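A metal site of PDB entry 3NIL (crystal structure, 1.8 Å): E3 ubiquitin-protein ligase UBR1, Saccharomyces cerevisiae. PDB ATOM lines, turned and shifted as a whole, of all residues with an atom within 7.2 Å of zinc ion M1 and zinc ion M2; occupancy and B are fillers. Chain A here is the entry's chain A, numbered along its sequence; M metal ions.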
ATOM      1  N   HIS A   4      36.340  -4.490  15.426  1.00  0.00           N
ATOM      2  CA  HIS A   4      36.010  -3.824  16.679  1.00  0.00           C
ATOM      3  C   HIS A   4      34.702  -4.381  17.224  1.00  0.00           C
ATOM      4  O   HIS A   4      33.730  -4.517  16.487  1.00  0.00           O
ATOM      5  CB  HIS A   4      35.918  -2.311  16.457  1.00  0.00           C
ATOM      6  CG  HIS A   4      35.798  -1.528  17.724  1.00  0.00           C
ATOM      7  ND1 HIS A   4      35.340  -0.230  17.751  1.00  0.00           N
ATOM      8  CD2 HIS A   4      36.093  -1.843  19.015  1.00  0.00           C
ATOM      9  CE1 HIS A   4      35.354   0.225  18.998  1.00  0.00           C
ATOM     10  NE2 HIS A   4      35.809  -0.735  19.776  1.00  0.00           N
ATOM     11  N   LYS A   5      34.708  -4.752  18.508  1.00  0.00           N
ATOM     12  CA  LYS A   5      33.508  -5.235  19.175  1.00  0.00           C
ATOM     13  C   LYS A   5      32.629  -4.038  19.545  1.00  0.00           C
ATOM     14  O   LYS A   5      33.119  -2.941  19.763  1.00  0.00           O
ATOM     15  CB  LYS A   5      33.869  -6.006  20.444  1.00  0.00           C
ATOM     16  CG  LYS A   5      34.746  -7.245  20.207  1.00  0.00           C
ATOM     17  CD  LYS A   5      35.005  -7.955  21.521  1.00  0.00           C
ATOM     18  CE  LYS A   5      35.994  -9.098  21.370  1.00  0.00           C
ATOM     19  NZ  LYS A   5      36.158  -9.795  22.693  1.00  0.00           N
ATOM     20  N   HIS A   6      31.317  -4.259  19.580  1.00  0.00           N
ATOM     21  CA  HIS A   6      30.380  -3.215  19.972  1.00  0.00           C
ATOM     22  C   HIS A   6      29.567  -3.656  21.187  1.00  0.00           C
ATOM     23  O   HIS A   6      28.360  -3.436  21.263  1.00  0.00           O
ATOM     24  CB  HIS A   6      29.470  -2.833  18.793  1.00  0.00           C
ATOM     25  CG  HIS A   6      28.611  -3.956  18.287  1.00  0.00           C
ATOM     26  ND1 HIS A   6      27.361  -4.215  18.798  1.00  0.00           N
ATOM     27  CD2 HIS A   6      28.813  -4.845  17.295  1.00  0.00           C
ATOM     28  CE1 HIS A   6      26.823  -5.238  18.143  1.00  0.00           C
ATOM     29  NE2 HIS A   6      27.691  -5.646  17.232  1.00  0.00           N
ATOM     30  N   ARG A   9      26.003  -2.454  23.083  1.00  0.00           N
ATOM     31  CA  ARG A   9      25.278  -1.522  22.211  1.00  0.00           C
ATOM     32  C   ARG A   9      25.060  -2.137  20.842  1.00  0.00           C
ATOM     33  O   ARG A   9      25.473  -3.260  20.584  1.00  0.00           O
ATOM     34  CB  ARG A   9      26.014  -0.175  22.070  1.00  0.00           C
ATOM     35  CG  ARG A   9      27.432  -0.278  21.520  1.00  0.00           C
ATOM     36  CD  ARG A   9      27.910   1.034  20.932  1.00  0.00           C
ATOM     37  NE  ARG A   9      27.503   1.188  19.530  1.00  0.00           N
ATOM     38  CZ  ARG A   9      27.866   2.193  18.744  1.00  0.00           C
ATOM     39  NH1 ARG A   9      28.639   3.180  19.199  1.00  0.00           N
ATOM     40  NH2 ARG A   9      27.450   2.215  17.491  1.00  0.00           N
ATOM     41  N   ASN A  10      24.395  -1.410  19.970  1.00  0.00           N
ATOM     42  CA  ASN A  10      24.158  -1.876  18.621  1.00  0.00           C
ATOM     43  C   ASN A  10      25.408  -1.652  17.785  1.00  0.00           C
ATOM     44  O   ASN A  10      26.298  -0.872  18.150  1.00  0.00           O
ATOM     45  CB  ASN A  10      22.986  -1.103  18.011  1.00  0.00           C
ATOM     46  CG  ASN A  10      23.334   0.322  17.758  1.00  0.00           C
ATOM     47  OD1 ASN A  10      23.735   1.043  18.672  1.00  0.00           O
ATOM     48  ND2 ASN A  10      23.218   0.756  16.518  1.00  0.00           N
ATOM     49  N   CYS A  11      25.487  -2.342  16.655  1.00  0.00           N
ATOM     50  CA  CYS A  11      26.581  -2.145  15.732  1.00  0.00           C
ATOM     51  C   CYS A  11      26.410  -0.790  15.012  1.00  0.00           C
ATOM     52  O   CYS A  11      27.238   0.134  15.158  1.00  0.00           O
ATOM     53  CB  CYS A  11      26.655  -3.329  14.762  1.00  0.00           C
ATOM     54  SG  CYS A  11      27.803  -3.044  13.424  1.00  0.00           S
ATOM     55  N   GLY A  12      25.347  -0.682  14.224  1.00  0.00           N
ATOM     56  CA  GLY A  12      25.045   0.551  13.504  1.00  0.00           C
ATOM     57  C   GLY A  12      26.011   0.942  12.391  1.00  0.00           C
ATOM     58  O   GLY A  12      25.929   2.053  11.865  1.00  0.00           O
ATOM     59  N   ARG A  13      26.920   0.049  12.015  1.00  0.00           N
ATOM     60  CA  ARG A  13      27.895   0.326  10.960  1.00  0.00           C
ATOM     61  C   ARG A  13      27.181   0.617   9.656  1.00  0.00           C
ATOM     62  O   ARG A  13      26.332  -0.157   9.224  1.00  0.00           O
ATOM     63  CB  ARG A  13      28.808  -0.898  10.782  1.00  0.00           C
ATOM     64  CG  ARG A  13      30.039  -0.672   9.941  1.00  0.00           C
ATOM     65  CD  ARG A  13      30.930  -1.907  10.004  1.00  0.00           C
ATOM     66  NE  ARG A  13      31.952  -1.919   8.956  1.00  0.00           N
ATOM     67  CZ  ARG A  13      31.716  -2.205   7.676  1.00  0.00           C
ATOM     68  NH1 ARG A  13      32.716  -2.206   6.809  1.00  0.00           N
ATOM     69  NH2 ARG A  13      30.487  -2.506   7.269  1.00  0.00           N
ATOM     70  N   PHE A  15      27.064   0.466   5.856  1.00  0.00           N
ATOM     71  CA  PHE A  15      27.660  -0.360   4.805  1.00  0.00           C
ATOM     72  C   PHE A  15      28.447   0.504   3.816  1.00  0.00           C
ATOM     73  O   PHE A  15      28.067   1.633   3.518  1.00  0.00           O
ATOM     74  CB  PHE A  15      26.576  -1.162   4.098  1.00  0.00           C
ATOM     75  CG  PHE A  15      25.917  -2.171   4.989  1.00  0.00           C
ATOM     76  CD1 PHE A  15      26.466  -3.438   5.160  1.00  0.00           C
ATOM     77  CD2 PHE A  15      24.751  -1.842   5.669  1.00  0.00           C
ATOM     78  CE1 PHE A  15      25.855  -4.367   5.995  1.00  0.00           C
ATOM     79  CE2 PHE A  15      24.131  -2.761   6.505  1.00  0.00           C
ATOM     80  CZ  PHE A  15      24.679  -4.028   6.677  1.00  0.00           C
ATOM     81  N   VAL A  34      19.112  -6.036   8.766  1.00  0.00           N
ATOM     82  CA  VAL A  34      20.356  -6.521   8.146  1.00  0.00           C
ATOM     83  C   VAL A  34      21.546  -6.628   9.105  1.00  0.00           C
ATOM     84  O   VAL A  34      21.548  -6.042  10.203  1.00  0.00           O
ATOM     85  CB  VAL A  34      20.769  -5.653   6.934  1.00  0.00           C
ATOM     86  CG1 VAL A  34      19.768  -5.844   5.787  1.00  0.00           C
ATOM     87  CG2 VAL A  34      20.920  -4.190   7.311  1.00  0.00           C
ATOM     88  N   LEU A  35      22.543  -7.399   8.663  1.00  0.00           N
ATOM     89  CA  LEU A  35      23.775  -7.626   9.432  1.00  0.00           C
ATOM     90  C   LEU A  35      24.992  -7.436   8.552  1.00  0.00           C
ATOM     91  O   LEU A  35      25.010  -7.856   7.387  1.00  0.00           O
ATOM     92  CB  LEU A  35      23.797  -9.067   9.986  1.00  0.00           C
ATOM     93  CG  LEU A  35      22.759  -9.314  11.083  1.00  0.00           C
ATOM     94  CD1 LEU A  35      22.583 -10.809  11.433  1.00  0.00           C
ATOM     95  CD2 LEU A  35      23.143  -8.525  12.323  1.00  0.00           C
ATOM     96  N   CYS A  36      26.022  -6.812   9.122  1.00  0.00           N
ATOM     97  CA  CYS A  36      27.261  -6.572   8.401  1.00  0.00           C
ATOM     98  C   CYS A  36      28.182  -7.787   8.511  1.00  0.00           C
ATOM     99  O   CYS A  36      27.924  -8.677   9.307  1.00  0.00           O
ATOM    100  CB  CYS A  36      27.965  -5.312   8.917  1.00  0.00           C
ATOM    101  SG  CYS A  36      28.864  -5.534  10.440  1.00  0.00           S
ATOM    102  N   ILE A  37      29.245  -7.799   7.710  1.00  0.00           N
ATOM    103  CA  ILE A  37      30.196  -8.935   7.684  1.00  0.00           C
ATOM    104  C   ILE A  37      31.029  -9.083   8.970  1.00  0.00           C
ATOM    105  O   ILE A  37      31.555 -10.146   9.265  1.00  0.00           O
ATOM    106  CB  ILE A  37      31.084  -8.920   6.395  1.00  0.00           C
ATOM    107  CG1 ILE A  37      31.785 -10.283   6.201  1.00  0.00           C
ATOM    108  CG2 ILE A  37      32.095  -7.766   6.415  1.00  0.00           C
ATOM    109  CD1 ILE A  37      32.110 -10.619   4.751  1.00  0.00           C
ATOM    110  N   HIS A  38      31.116  -8.001   9.747  1.00  0.00           N
ATOM    111  CA  HIS A  38      31.779  -8.038  11.047  1.00  0.00           C
ATOM    112  C   HIS A  38      30.942  -8.835  12.056  1.00  0.00           C
ATOM    113  O   HIS A  38      31.490  -9.477  12.971  1.00  0.00           O
ATOM    114  CB  HIS A  38      31.980  -6.612  11.592  1.00  0.00           C
ATOM    115  CG  HIS A  38      32.824  -5.736  10.729  1.00  0.00           C
ATOM    116  ND1 HIS A  38      33.404  -4.581  11.197  1.00  0.00           N
ATOM    117  CD2 HIS A  38      33.189  -5.838   9.418  1.00  0.00           C
ATOM    118  CE1 HIS A  38      34.088  -3.997  10.225  1.00  0.00           C
ATOM    119  NE2 HIS A  38      33.969  -4.742   9.135  1.00  0.00           N
ATOM    120  N   CYS A  39      29.627  -8.792  11.867  1.00  0.00           N
ATOM    121  CA  CYS A  39      28.679  -9.261  12.856  1.00  0.00           C
ATOM    122  C   CYS A  39      28.022 -10.595  12.534  1.00  0.00           C
ATOM    123  O   CYS A  39      27.772 -11.390  13.448  1.00  0.00           O
ATOM    124  CB  CYS A  39      27.589  -8.210  13.060  1.00  0.00           C
ATOM    125  SG  CYS A  39      28.247  -6.773  13.869  1.00  0.00           S
ATOM    126  N   PHE A  40      27.697 -10.801  11.267  1.00  0.00           N
ATOM    127  CA  PHE A  40      26.953 -11.987  10.841  1.00  0.00           C
ATOM    128  C   PHE A  40      27.697 -13.244  11.275  1.00  0.00           C
ATOM    129  O   PHE A  40      28.891 -13.394  10.991  1.00  0.00           O
ATOM    130  CB  PHE A  40      26.715 -11.987   9.339  1.00  0.00           C
ATOM    131  CG  PHE A  40      26.029 -13.232   8.838  1.00  0.00           C
ATOM    132  CD1 PHE A  40      24.640 -13.313   8.841  1.00  0.00           C
ATOM    133  CD2 PHE A  40      26.773 -14.316   8.338  1.00  0.00           C
ATOM    134  CE1 PHE A  40      23.990 -14.455   8.366  1.00  0.00           C
ATOM    135  CE2 PHE A  40      26.129 -15.456   7.879  1.00  0.00           C
ATOM    136  CZ  PHE A  40      24.737 -15.541   7.889  1.00  0.00           C
ATOM    137  N   ILE A  62      22.467   0.576   7.662  1.00  0.00           N
ATOM    138  CA  ILE A  62      23.283   0.326   8.822  1.00  0.00           C
ATOM    139  C   ILE A  62      22.937  -1.044   9.401  1.00  0.00           C
ATOM    140  O   ILE A  62      21.808  -1.548   9.241  1.00  0.00           O
ATOM    141  CB  ILE A  62      23.106   1.412   9.915  1.00  0.00           C
ATOM    142  CG1 ILE A  62      21.644   1.475  10.388  1.00  0.00           C
ATOM    143  CG2 ILE A  62      23.593   2.781   9.389  1.00  0.00           C
ATOM    144  CD1 ILE A  62      21.496   1.384  11.876  1.00  0.00           C
ATOM    145  N   CYS A  63      23.935  -1.627  10.069  1.00  0.00           N
ATOM    146  CA  CYS A  63      23.836  -2.965  10.613  1.00  0.00           C
ATOM    147  C   CYS A  63      23.016  -2.950  11.896  1.00  0.00           C
ATOM    148  O   CYS A  63      23.184  -2.074  12.740  1.00  0.00           O
ATOM    149  CB  CYS A  63      25.257  -3.516  10.874  1.00  0.00           C
ATOM    150  SG  CYS A  63      25.279  -5.043  11.803  1.00  0.00           S
ATOM    151  N   ASP A  64      22.091  -3.916  12.018  1.00  0.00           N
ATOM    152  CA  ASP A  64      21.150  -3.981  13.149  1.00  0.00           C
ATOM    153  C   ASP A  64      21.574  -4.941  14.269  1.00  0.00           C
ATOM    154  O   ASP A  64      20.823  -5.167  15.231  1.00  0.00           O
ATOM    155  CB  ASP A  64      19.742  -4.367  12.673  1.00  0.00           C
ATOM    156  CG  ASP A  64      19.182  -3.391  11.657  1.00  0.00           C
ATOM    157  OD1 ASP A  64      19.132  -2.164  11.942  1.00  0.00           O
ATOM    158  OD2 ASP A  64      18.786  -3.846  10.559  1.00  0.00           O
ATOM    159  N   CYS A  65      22.764  -5.528  14.167  1.00  0.00           N
ATOM    160  CA  CYS A  65      23.259  -6.405  15.229  1.00  0.00           C
ATOM    161  C   CYS A  65      23.230  -5.692  16.586  1.00  0.00           C
ATOM    162  O   CYS A  65      23.711  -4.564  16.708  1.00  0.00           O
ATOM    163  CB  CYS A  65      24.684  -6.858  14.891  1.00  0.00           C
ATOM    164  SG  CYS A  65      25.404  -8.019  16.066  1.00  0.00           S
ATOM    165  N   GLY A  66      22.675  -6.346  17.590  1.00  0.00           N
ATOM    166  CA  GLY A  66      22.594  -5.761  18.925  1.00  0.00           C
ATOM    167  C   GLY A  66      21.502  -4.717  19.101  1.00  0.00           C
ATOM    168  O   GLY A  66      21.430  -4.084  20.151  1.00  0.00           O
ATOM    169  N   LEU A  75      21.151 -13.149  18.723  1.00  0.00           N
ATOM    170  CA  LEU A  75      22.330 -13.278  17.873  1.00  0.00           C
ATOM    171  C   LEU A  75      23.565 -13.367  18.724  1.00  0.00           C
ATOM    172  O   LEU A  75      23.608 -12.854  19.833  1.00  0.00           O
ATOM    173  CB  LEU A  75      22.501 -12.080  16.933  1.00  0.00           C
ATOM    174  CG  LEU A  75      21.343 -11.753  15.994  1.00  0.00           C
ATOM    175  CD1 LEU A  75      21.746 -10.588  15.110  1.00  0.00           C
ATOM    176  CD2 LEU A  75      20.996 -12.971  15.150  1.00  0.00           C
ATOM    177  N   HIS A  76      24.596 -13.997  18.159  1.00  0.00           N
ATOM    178  CA  HIS A  76      25.898 -14.095  18.787  1.00  0.00           C
ATOM    179  C   HIS A  76      26.876 -13.434  17.848  1.00  0.00           C
ATOM    180  O   HIS A  76      27.417 -14.062  16.953  1.00  0.00           O
ATOM    181  CB  HIS A  76      26.252 -15.557  19.002  1.00  0.00           C
ATOM    182  CG  HIS A  76      25.237 -16.274  19.833  1.00  0.00           C
ATOM    183  ND1 HIS A  76      24.231 -17.027  19.269  1.00  0.00           N
ATOM    184  CD2 HIS A  76      25.038 -16.303  21.166  1.00  0.00           C
ATOM    185  CE1 HIS A  76      23.467 -17.517  20.230  1.00  0.00           C
ATOM    186  NE2 HIS A  76      23.934 -17.096  21.395  1.00  0.00           N
ATOM    187  N   CYS A  77      27.051 -12.132  18.043  1.00  0.00           N
ATOM    188  CA  CYS A  77      27.861 -11.337  17.156  1.00  0.00           C
ATOM    189  C   CYS A  77      29.203 -12.021  16.895  1.00  0.00           C
ATOM    190  O   CYS A  77      29.883 -12.420  17.819  1.00  0.00           O
ATOM    191  CB  CYS A  77      28.098  -9.967  17.804  1.00  0.00           C
ATOM    192  SG  CYS A  77      29.139  -8.834  16.849  1.00  0.00           S
ATOM    193  N   LYS A  78      29.575 -12.153  15.618  1.00  0.00           N
ATOM    194  CA  LYS A  78      30.862 -12.770  15.253  1.00  0.00           C
ATOM    195  C   LYS A  78      32.075 -12.065  15.879  1.00  0.00           C
ATOM    196  O   LYS A  78      33.058 -12.725  16.253  1.00  0.00           O
ATOM    197  CB  LYS A  78      31.008 -12.866  13.730  1.00  0.00           C
ATOM    198  CG  LYS A  78      32.117 -13.806  13.231  1.00  0.00           C
ATOM    199  CD  LYS A  78      32.024 -13.958  11.706  1.00  0.00           C
ATOM    200  CE  LYS A  78      32.878 -15.094  11.204  1.00  0.00           C
ATOM    201  NZ  LYS A  78      34.311 -14.837  11.443  1.00  0.00           N
ATOM    202  N   ALA A  79      32.010 -10.739  16.010  1.00  0.00           N
ATOM    203  CA  ALA A  79      33.123  -9.970  16.575  1.00  0.00           C
ATOM    204  C   ALA A  79      33.499 -10.385  18.008  1.00  0.00           C
ATOM    205  O   ALA A  79      34.641 -10.208  18.444  1.00  0.00           O
ATOM    206  CB  ALA A  79      32.835  -8.462  16.509  1.00  0.00           C
ATOM    207  N   GLU A  80      32.536 -10.945  18.731  1.00  0.00           N
ATOM    208  CA  GLU A  80      32.780 -11.361  20.115  1.00  0.00           C
ATOM    209  C   GLU A  80      33.606 -12.645  20.198  1.00  0.00           C
ATOM    210  O   GLU A  80      34.173 -12.953  21.254  1.00  0.00           O
ATOM    211  CB  GLU A  80      31.450 -11.543  20.848  1.00  0.00           C
ATOM    212  CG  GLU A  80      30.600 -10.271  20.907  1.00  0.00           C
ATOM    213  CD  GLU A  80      31.115  -9.253  21.916  1.00  0.00           C
ATOM    214  OE1 GLU A  80      31.886  -9.638  22.822  1.00  0.00           O
ATOM    215  OE2 GLU A  80      30.739  -8.066  21.799  1.00  0.00           O
HETATM  216 ZN    ZN M   1      27.544  -5.025  12.289  1.00  0.00          ZN
HETATM  217 ZN    ZN M   2      27.636  -7.367  16.021  1.00  0.00          ZN
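The nearest printed residue that does not touch zinc ion M2 is Cys 11 (4.3 Å).
The nearest printed residue that does not touch zinc ion M1 is Cys 65 (4.3 Å).
The backbone carbonyl oxygen of Arg 9 sits at hydrogen-bond distance from a ring nitrogen (ND1) of His 6, 2.8 Å away. N of Ala 79 sits close to SG of Cys 77 (3.5 Å). N of Cys 11 is in hydrogen-bond range of O of Cys 65 (2.8 Å). The side-chain sulfur (SG) of Cys 11 lies close to the backbone NH (N) of Arg 13 (3.5 Å). The guanidinium group of Arg 9 is in hydrogen-bond range of the backbone carbonyl oxygen of Cys 11. The backbone NH of Lys 78 sits at hydrogen-bond distance from the backbone carbonyl oxygen of Cys 39 (2.9 Å). N of Cys 63 lies within hydrogen-bond range of O of Arg 13 (2.9 Å). The backbone NH (N) of Gly 12 is in hydrogen-bond range of the backbone carbonyl oxygen (O) of Cys 63, 3.0 Å away.
Zinc ion M1 is bound by SG of Cys 11, SG of Cys 63, SG of Cys 36 and SG of Cys 39. Zinc ion M1 has four donor atoms within binding distance.
Zinc ion M2 is bound by a ring nitrogen (NE2) of His 6 (2.1 Å). The side-chain sulfur (SG) of Cys 77 binds zinc ion M2 (2.3 Å). Zinc ion M2 is bound by the side-chain sulfur (SG) of Cys 39. Zinc ion M2 is bound by the side-chain sulfur (SG) of Cys 65, 2.3 Å away.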
